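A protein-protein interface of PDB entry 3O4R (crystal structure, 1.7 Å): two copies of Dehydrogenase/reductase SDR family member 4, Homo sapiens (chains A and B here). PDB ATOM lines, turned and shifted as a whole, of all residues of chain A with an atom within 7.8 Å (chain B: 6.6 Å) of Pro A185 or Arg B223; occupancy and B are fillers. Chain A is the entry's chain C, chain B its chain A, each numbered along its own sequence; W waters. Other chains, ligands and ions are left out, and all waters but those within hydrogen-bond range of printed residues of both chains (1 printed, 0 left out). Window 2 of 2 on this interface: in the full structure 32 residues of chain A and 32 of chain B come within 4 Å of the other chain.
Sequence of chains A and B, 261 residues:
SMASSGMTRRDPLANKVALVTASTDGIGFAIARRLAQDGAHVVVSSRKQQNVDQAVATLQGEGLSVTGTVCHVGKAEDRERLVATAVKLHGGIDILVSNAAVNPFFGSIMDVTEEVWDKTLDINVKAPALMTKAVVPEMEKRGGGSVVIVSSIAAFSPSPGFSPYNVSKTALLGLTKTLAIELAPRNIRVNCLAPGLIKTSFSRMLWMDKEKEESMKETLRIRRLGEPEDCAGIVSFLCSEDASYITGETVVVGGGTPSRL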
ATOM      1  N   GLU A 140      31.066 -26.243 -20.036  1.00  0.00           N
ATOM      2  CA  GLU A 140      29.721 -25.967 -20.546  1.00  0.00           C
ATOM      3  C   GLU A 140      28.777 -27.142 -20.397  1.00  0.00           C
ATOM      4  O   GLU A 140      27.598 -26.959 -20.105  1.00  0.00           O
ATOM      5  CB  GLU A 140      29.782 -25.622 -22.028  1.00  0.00           C
ATOM      6  CG  GLU A 140      29.961 -24.184 -22.335  1.00  0.00           C
ATOM      7  CD  GLU A 140      29.900 -23.935 -23.820  1.00  0.00           C
ATOM      8  OE1 GLU A 140      29.014 -23.180 -24.264  1.00  0.00           O
ATOM      9  OE2 GLU A 140      30.736 -24.514 -24.546  1.00  0.00           O
ATOM     10  N   GLY A 143      27.426 -27.642 -16.886  1.00  0.00           N
ATOM     11  CA  GLY A 143      26.605 -26.532 -16.399  1.00  0.00           C
ATOM     12  C   GLY A 143      27.423 -25.359 -15.881  1.00  0.00           C
ATOM     13  O   GLY A 143      26.866 -24.382 -15.364  1.00  0.00           O
ATOM     14  N   LEU A 179      38.757 -12.948 -19.165  1.00  0.00           N
ATOM     15  CA  LEU A 179      38.121 -14.249 -19.223  1.00  0.00           C
ATOM     16  C   LEU A 179      36.924 -14.383 -18.300  1.00  0.00           C
ATOM     17  O   LEU A 179      35.983 -15.089 -18.642  1.00  0.00           O
ATOM     18  CB  LEU A 179      39.099 -15.374 -18.865  1.00  0.00           C
ATOM     19  CG  LEU A 179      40.265 -15.688 -19.794  1.00  0.00           C
ATOM     20  CD1 LEU A 179      40.976 -16.893 -19.203  1.00  0.00           C
ATOM     21  CD2 LEU A 179      39.785 -15.959 -21.209  1.00  0.00           C
ATOM     22  N   ALA A 180      36.972 -13.757 -17.123  1.00  0.00           N
ATOM     23  CA  ALA A 180      35.840 -13.805 -16.191  1.00  0.00           C
ATOM     24  C   ALA A 180      34.626 -13.137 -16.855  1.00  0.00           C
ATOM     25  O   ALA A 180      33.510 -13.631 -16.746  1.00  0.00           O
ATOM     26  CB  ALA A 180      36.186 -13.121 -14.835  1.00  0.00           C
ATOM     27  N   ILE A 181      34.852 -12.036 -17.560  1.00  0.00           N
ATOM     28  CA  ILE A 181      33.749 -11.366 -18.252  1.00  0.00           C
ATOM     29  C   ILE A 181      33.283 -12.217 -19.446  1.00  0.00           C
ATOM     30  O   ILE A 181      32.084 -12.438 -19.615  1.00  0.00           O
ATOM     31  CB  ILE A 181      34.123  -9.951 -18.725  1.00  0.00           C
ATOM     32  CG1 ILE A 181      34.465  -9.052 -17.541  1.00  0.00           C
ATOM     33  CG2 ILE A 181      32.946  -9.306 -19.461  1.00  0.00           C
ATOM     34  CD1 ILE A 181      34.812  -7.610 -17.947  1.00  0.00           C
ATOM     35  N   GLU A 182      34.231 -12.712 -20.247  1.00  0.00           N
ATOM     36  CA  GLU A 182      33.907 -13.516 -21.431  1.00  0.00           C
ATOM     37  C   GLU A 182      33.111 -14.775 -21.093  1.00  0.00           C
ATOM     38  O   GLU A 182      32.167 -15.116 -21.789  1.00  0.00           O
ATOM     39  CB  GLU A 182      35.180 -13.943 -22.170  1.00  0.00           C
ATOM     40  CG  GLU A 182      35.899 -12.822 -22.905  1.00  0.00           C
ATOM     41  CD  GLU A 182      35.947 -12.985 -24.423  1.00  0.00           C
ATOM     42  OE1 GLU A 182      35.526 -14.030 -24.960  1.00  0.00           O
ATOM     43  OE2 GLU A 182      36.440 -12.040 -25.075  1.00  0.00           O
ATOM     44  N   LEU A 183      33.499 -15.463 -20.028  1.00  0.00           N
ATOM     45  CA  LEU A 183      32.973 -16.784 -19.749  1.00  0.00           C
ATOM     46  C   LEU A 183      31.836 -16.831 -18.735  1.00  0.00           C
ATOM     47  O   LEU A 183      31.328 -17.912 -18.435  1.00  0.00           O
ATOM     48  CB  LEU A 183      34.105 -17.686 -19.285  1.00  0.00           C
ATOM     49  CG  LEU A 183      35.287 -17.888 -20.246  1.00  0.00           C
ATOM     50  CD1 LEU A 183      36.282 -18.854 -19.615  1.00  0.00           C
ATOM     51  CD2 LEU A 183      34.840 -18.424 -21.617  1.00  0.00           C
ATOM     52  N   ALA A 184      31.423 -15.669 -18.230  1.00  0.00           N
ATOM     53  CA  ALA A 184      30.340 -15.590 -17.250  1.00  0.00           C
ATOM     54  C   ALA A 184      29.000 -16.129 -17.800  1.00  0.00           C
ATOM     55  O   ALA A 184      28.307 -16.843 -17.082  1.00  0.00           O
ATOM     56  CB  ALA A 184      30.180 -14.171 -16.748  1.00  0.00           C
ATOM     57  N   PRO A 185      28.646 -15.811 -19.071  1.00  0.00           N
ATOM     58  CA  PRO A 185      27.413 -16.400 -19.637  1.00  0.00           C
ATOM     59  C   PRO A 185      27.389 -17.947 -19.659  1.00  0.00           C
ATOM     60  O   PRO A 185      26.313 -18.533 -19.584  1.00  0.00           O
ATOM     61  CB  PRO A 185      27.354 -15.812 -21.042  1.00  0.00           C
ATOM     62  CG  PRO A 185      28.101 -14.512 -20.932  1.00  0.00           C
ATOM     63  CD  PRO A 185      29.251 -14.841 -19.999  1.00  0.00           C
ATOM     64  N   ARG A 186      28.552 -18.593 -19.708  1.00  0.00           N
ATOM     65  CA  ARG A 186      28.622 -20.056 -19.579  1.00  0.00           C
ATOM     66  C   ARG A 186      28.677 -20.562 -18.136  1.00  0.00           C
ATOM     67  O   ARG A 186      28.896 -21.767 -17.912  1.00  0.00           O
ATOM     68  CB  ARG A 186      29.836 -20.608 -20.345  1.00  0.00           C
ATOM     69  CG  ARG A 186      29.841 -20.363 -21.862  1.00  0.00           C
ATOM     70  CD  ARG A 186      31.206 -20.746 -22.438  1.00  0.00           C
ATOM     71  NE  ARG A 186      31.203 -20.946 -23.890  1.00  0.00           N
ATOM     72  CZ  ARG A 186      31.460 -20.007 -24.798  1.00  0.00           C
ATOM     73  NH1 ARG A 186      31.740 -18.763 -24.439  1.00  0.00           N
ATOM     74  NH2 ARG A 186      31.428 -20.322 -26.089  1.00  0.00           N
ATOM     75  N   ASN A 187      28.466 -19.672 -17.160  1.00  0.00           N
ATOM     76  CA  ASN A 187      28.563 -20.036 -15.740  1.00  0.00           C
ATOM     77  C   ASN A 187      29.951 -20.572 -15.378  1.00  0.00           C
ATOM     78  O   ASN A 187      30.081 -21.495 -14.561  1.00  0.00           O
ATOM     79  CB  ASN A 187      27.481 -21.077 -15.368  1.00  0.00           C
ATOM     80  CG  ASN A 187      27.215 -21.138 -13.855  1.00  0.00           C
ATOM     81  OD1 ASN A 187      27.194 -20.114 -13.190  1.00  0.00           O
ATOM     82  ND2 ASN A 187      27.021 -22.337 -13.321  1.00  0.00           N
ATOM     83  N   ILE A 188      30.985 -20.048 -16.025  1.00  0.00           N
ATOM     84  CA  ILE A 188      32.346 -20.399 -15.669  1.00  0.00           C
ATOM     85  C   ILE A 188      32.957 -19.217 -14.923  1.00  0.00           C
ATOM     86  O   ILE A 188      32.955 -18.083 -15.431  1.00  0.00           O
ATOM     87  CB  ILE A 188      33.191 -20.776 -16.885  1.00  0.00           C
ATOM     88  CG1 ILE A 188      32.677 -22.073 -17.518  1.00  0.00           C
ATOM     89  CG2 ILE A 188      34.650 -20.918 -16.502  1.00  0.00           C
ATOM     90  CD1 ILE A 188      33.218 -22.300 -18.939  1.00  0.00           C
ATOM     91  N   SER A 244      30.420 -19.037  -5.331  1.00  0.00           N
ATOM     92  CA  SER A 244      29.685 -18.829  -6.606  1.00  0.00           C
ATOM     93  C   SER A 244      29.502 -17.368  -6.952  1.00  0.00           C
ATOM     94  O   SER A 244      29.241 -17.023  -8.107  1.00  0.00           O
ATOM     95  CB  SER A 244      28.316 -19.528  -6.607  1.00  0.00           C
ATOM     96  OG  SER A 244      27.433 -18.988  -5.652  1.00  0.00           O
ATOM     97  N   TYR A 245      29.661 -16.504  -5.963  1.00  0.00           N
ATOM     98  CA  TYR A 245      29.538 -15.055  -6.218  1.00  0.00           C
ATOM     99  C   TYR A 245      30.890 -14.324  -6.294  1.00  0.00           C
ATOM    100  O   TYR A 245      30.957 -13.075  -6.304  1.00  0.00           O
ATOM    101  CB  TYR A 245      28.590 -14.427  -5.212  1.00  0.00           C
ATOM    102  CG  TYR A 245      27.877 -13.240  -5.797  1.00  0.00           C
ATOM    103  CD1 TYR A 245      27.077 -13.390  -6.920  1.00  0.00           C
ATOM    104  CD2 TYR A 245      28.019 -11.977  -5.250  1.00  0.00           C
ATOM    105  CE1 TYR A 245      26.416 -12.304  -7.479  1.00  0.00           C
ATOM    106  CE2 TYR A 245      27.365 -10.894  -5.805  1.00  0.00           C
ATOM    107  CZ  TYR A 245      26.571 -11.066  -6.918  1.00  0.00           C
ATOM    108  OH  TYR A 245      25.920  -9.988  -7.485  1.00  0.00           O
ATOM    109  N   THR A 247      34.021 -14.038  -8.909  1.00  0.00           N
ATOM    110  CA  THR A 247      34.656 -14.259 -10.208  1.00  0.00           C
ATOM    111  C   THR A 247      35.339 -12.970 -10.597  1.00  0.00           C
ATOM    112  O   THR A 247      34.892 -11.897 -10.154  1.00  0.00           O
ATOM    113  CB  THR A 247      33.640 -14.698 -11.311  1.00  0.00           C
ATOM    114  OG1 THR A 247      34.366 -15.136 -12.469  1.00  0.00           O
ATOM    115  CG2 THR A 247      32.691 -13.547 -11.717  1.00  0.00           C
ATOM    116  N   LYS B 217      21.344  -4.980 -12.509  1.00  0.00           N
ATOM    117  CA  LYS B 217      22.123  -6.095 -13.072  1.00  0.00           C
ATOM    118  C   LYS B 217      22.862  -5.683 -14.350  1.00  0.00           C
ATOM    119  O   LYS B 217      24.037  -6.018 -14.539  1.00  0.00           O
ATOM    120  CB  LYS B 217      21.225  -7.307 -13.374  1.00  0.00           C
ATOM    121  CG  LYS B 217      20.710  -8.048 -12.143  1.00  0.00           C
ATOM    122  CD  LYS B 217      19.463  -8.883 -12.440  1.00  0.00           C
ATOM    123  CE  LYS B 217      19.793 -10.179 -13.171  1.00  0.00           C
ATOM    124  NZ  LYS B 217      18.597 -11.063 -13.342  1.00  0.00           N
ATOM    125  N   ARG B 221      26.787  -5.266 -14.572  1.00  0.00           N
ATOM    126  CA  ARG B 221      27.355  -6.311 -15.436  1.00  0.00           C
ATOM    127  C   ARG B 221      27.404  -7.633 -14.686  1.00  0.00           C
ATOM    128  O   ARG B 221      28.413  -8.348 -14.685  1.00  0.00           O
ATOM    129  CB  ARG B 221      28.748  -5.926 -15.966  1.00  0.00           C
ATOM    130  CG  ARG B 221      28.736  -4.931 -17.123  1.00  0.00           C
ATOM    131  CD  ARG B 221      28.448  -3.529 -16.650  1.00  0.00           C
ATOM    132  NE  ARG B 221      28.727  -2.502 -17.659  1.00  0.00           N
ATOM    133  CZ  ARG B 221      29.943  -2.058 -17.988  1.00  0.00           C
ATOM    134  NH1 ARG B 221      31.038  -2.551 -17.412  1.00  0.00           N
ATOM    135  NH2 ARG B 221      30.067  -1.117 -18.916  1.00  0.00           N
ATOM    136  N   ILE B 222      26.287  -7.945 -14.052  1.00  0.00           N
ATOM    137  CA  ILE B 222      26.151  -9.141 -13.240  1.00  0.00           C
ATOM    138  C   ILE B 222      24.958  -9.958 -13.716  1.00  0.00           C
ATOM    139  O   ILE B 222      23.994  -9.417 -14.272  1.00  0.00           O
ATOM    140  CB  ILE B 222      25.997  -8.794 -11.738  1.00  0.00           C
ATOM    141  CG1 ILE B 222      24.855  -7.784 -11.494  1.00  0.00           C
ATOM    142  CG2 ILE B 222      27.311  -8.226 -11.186  1.00  0.00           C
ATOM    143  CD1 ILE B 222      24.704  -7.338 -10.024  1.00  0.00           C
ATOM    144  N   ARG B 223      25.028 -11.264 -13.472  1.00  0.00           N
ATOM    145  CA  ARG B 223      23.982 -12.195 -13.847  1.00  0.00           C
ATOM    146  C   ARG B 223      22.925 -12.389 -12.758  1.00  0.00           C
ATOM    147  O   ARG B 223      21.820 -12.828 -13.047  1.00  0.00           O
ATOM    148  CB  ARG B 223      24.604 -13.551 -14.189  1.00  0.00           C
ATOM    149  CG  ARG B 223      25.542 -13.502 -15.369  1.00  0.00           C
ATOM    150  CD  ARG B 223      26.149 -14.869 -15.637  1.00  0.00           C
ATOM    151  NE  ARG B 223      25.180 -15.753 -16.282  1.00  0.00           N
ATOM    152  CZ  ARG B 223      24.885 -16.995 -15.904  1.00  0.00           C
ATOM    153  NH1 ARG B 223      25.491 -17.572 -14.874  1.00  0.00           N
ATOM    154  NH2 ARG B 223      23.972 -17.675 -16.587  1.00  0.00           N
ATOM    155  N   ARG B 224      23.290 -12.111 -11.504  1.00  0.00           N
ATOM    156  CA  ARG B 224      22.364 -12.175 -10.379  1.00  0.00           C
ATOM    157  C   ARG B 224      22.852 -11.281  -9.249  1.00  0.00           C
ATOM    158  O   ARG B 224      24.046 -10.998  -9.158  1.00  0.00           O
ATOM    159  CB  ARG B 224      22.238 -13.620  -9.863  1.00  0.00           C
ATOM    160  CG  ARG B 224      23.476 -14.195  -9.176  1.00  0.00           C
ATOM    161  CD  ARG B 224      23.184 -15.548  -8.628  1.00  0.00           C
ATOM    162  NE  ARG B 224      24.330 -16.185  -7.975  1.00  0.00           N
ATOM    163  CZ  ARG B 224      24.706 -15.995  -6.706  1.00  0.00           C
ATOM    164  NH1 ARG B 224      24.054 -15.148  -5.915  1.00  0.00           N
ATOM    165  NH2 ARG B 224      25.759 -16.659  -6.225  1.00  0.00           N
ATOM    166  N   LEU B 225      21.934 -10.859  -8.382  1.00  0.00           N
ATOM    167  CA  LEU B 225      22.304 -10.190  -7.136  1.00  0.00           C
ATOM    168  C   LEU B 225      22.831 -11.223  -6.157  1.00  0.00           C
ATOM    169  O   LEU B 225      22.484 -12.410  -6.232  1.00  0.00           O
ATOM    170  CB  LEU B 225      21.121  -9.421  -6.521  1.00  0.00           C
ATOM    171  CG  LEU B 225      20.879  -7.996  -7.024  1.00  0.00           C
ATOM    172  CD1 LEU B 225      20.612  -7.989  -8.507  1.00  0.00           C
ATOM    173  CD2 LEU B 225      19.726  -7.338  -6.279  1.00  0.00           C
ATOM    174  N   GLY B 255      30.100 -10.949  -7.737  1.00  0.00           N
ATOM    175  CA  GLY B 255      29.537 -11.636  -8.906  1.00  0.00           C
ATOM    176  C   GLY B 255      30.079 -11.179 -10.252  1.00  0.00           C
ATOM    177  O   GLY B 255      29.431 -11.368 -11.285  1.00  0.00           O
HETATM  178  O   HOH W   1      26.158 -17.976  -8.829  1.00  0.00           O
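O of Pro A185 touches NH2 of Arg B223, 3.9 Å away.
OH of Tyr A245 touches CD1 of Ile B222, at 3.9 Å.
Tyr A245 touches Leu B225.
Gly B255 touches Thr A247.
Water W1 lies within hydrogen-bond range of the guanidinium group (NE) of Arg B224 (2.7 Å) and the backbone carbonyl oxygen (O) of Ser A244 (3.3 Å).
Pro A185 touches just one residue of chain B: Arg B223 (3.9 Å).
Of the printed residues of chain A, Gly B255 touches Tyr A245 (2.7 Å) and Thr A247 (3.8 Å).
Of the printed residues of chain B, Ala A184 touches Arg B223 (3.3 Å).
Printed residues of chain B within 4 Å of Ser A244: Arg B224 (2.9 Å).
Of the printed residues of chain A, Ile B222 touches Tyr A245 (3.9 Å).
The nearest residue of chain A that does not touch Arg B223 is Arg A186 (5.5 Å).
No position is printed for both chains.
Of the 9 pairs that touch across the chains among the printed residues, none has its exchanged pair printed and touching as well.
Printed residues of chain A that touch a printed residue of chain B: Ala A184, Pro A185, Asn A187, Ser A244, Tyr A245 and Thr A247.
Hydrophobic or aromatic side chains of chain A that line the printed part of chain B: Tyr A245.
Among the printed residues, 9 pairs touch across the chains.
Among the printed residues, no Asp or Glu carboxylate lies within 4 Å of a Lys or Arg side-chain nitrogen of the other chain.
The backbone carbonyl oxygen of Lys B217 is in hydrogen-bond range of the backbone NH of Ile B222 (3.0 Å).
The backbone carbonyl oxygen of Gly A143 is in hydrogen-bond range of the side-chain amide nitrogen of Asn A187 (2.9 Å).
The guanidinium group (NE) of Arg B223 sits close to the backbone carbonyl oxygen (O) of Ala A184 (3.4 Å).
The side-chain amide oxygen (OD1) of Asn A187 sits at hydrogen-bond distance from the guanidinium group (NH1) of Arg B223.
The guanidinium group of Arg B224 is in hydrogen-bond range of the side-chain hydroxyl of Ser A244 (2.9 Å).
O of Arg B224 lies within hydrogen-bond range of OH of Tyr A245 (2.7 Å).
O of Tyr A245 is in hydrogen-bond range of N of Gly B255, 2.7 Å away.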
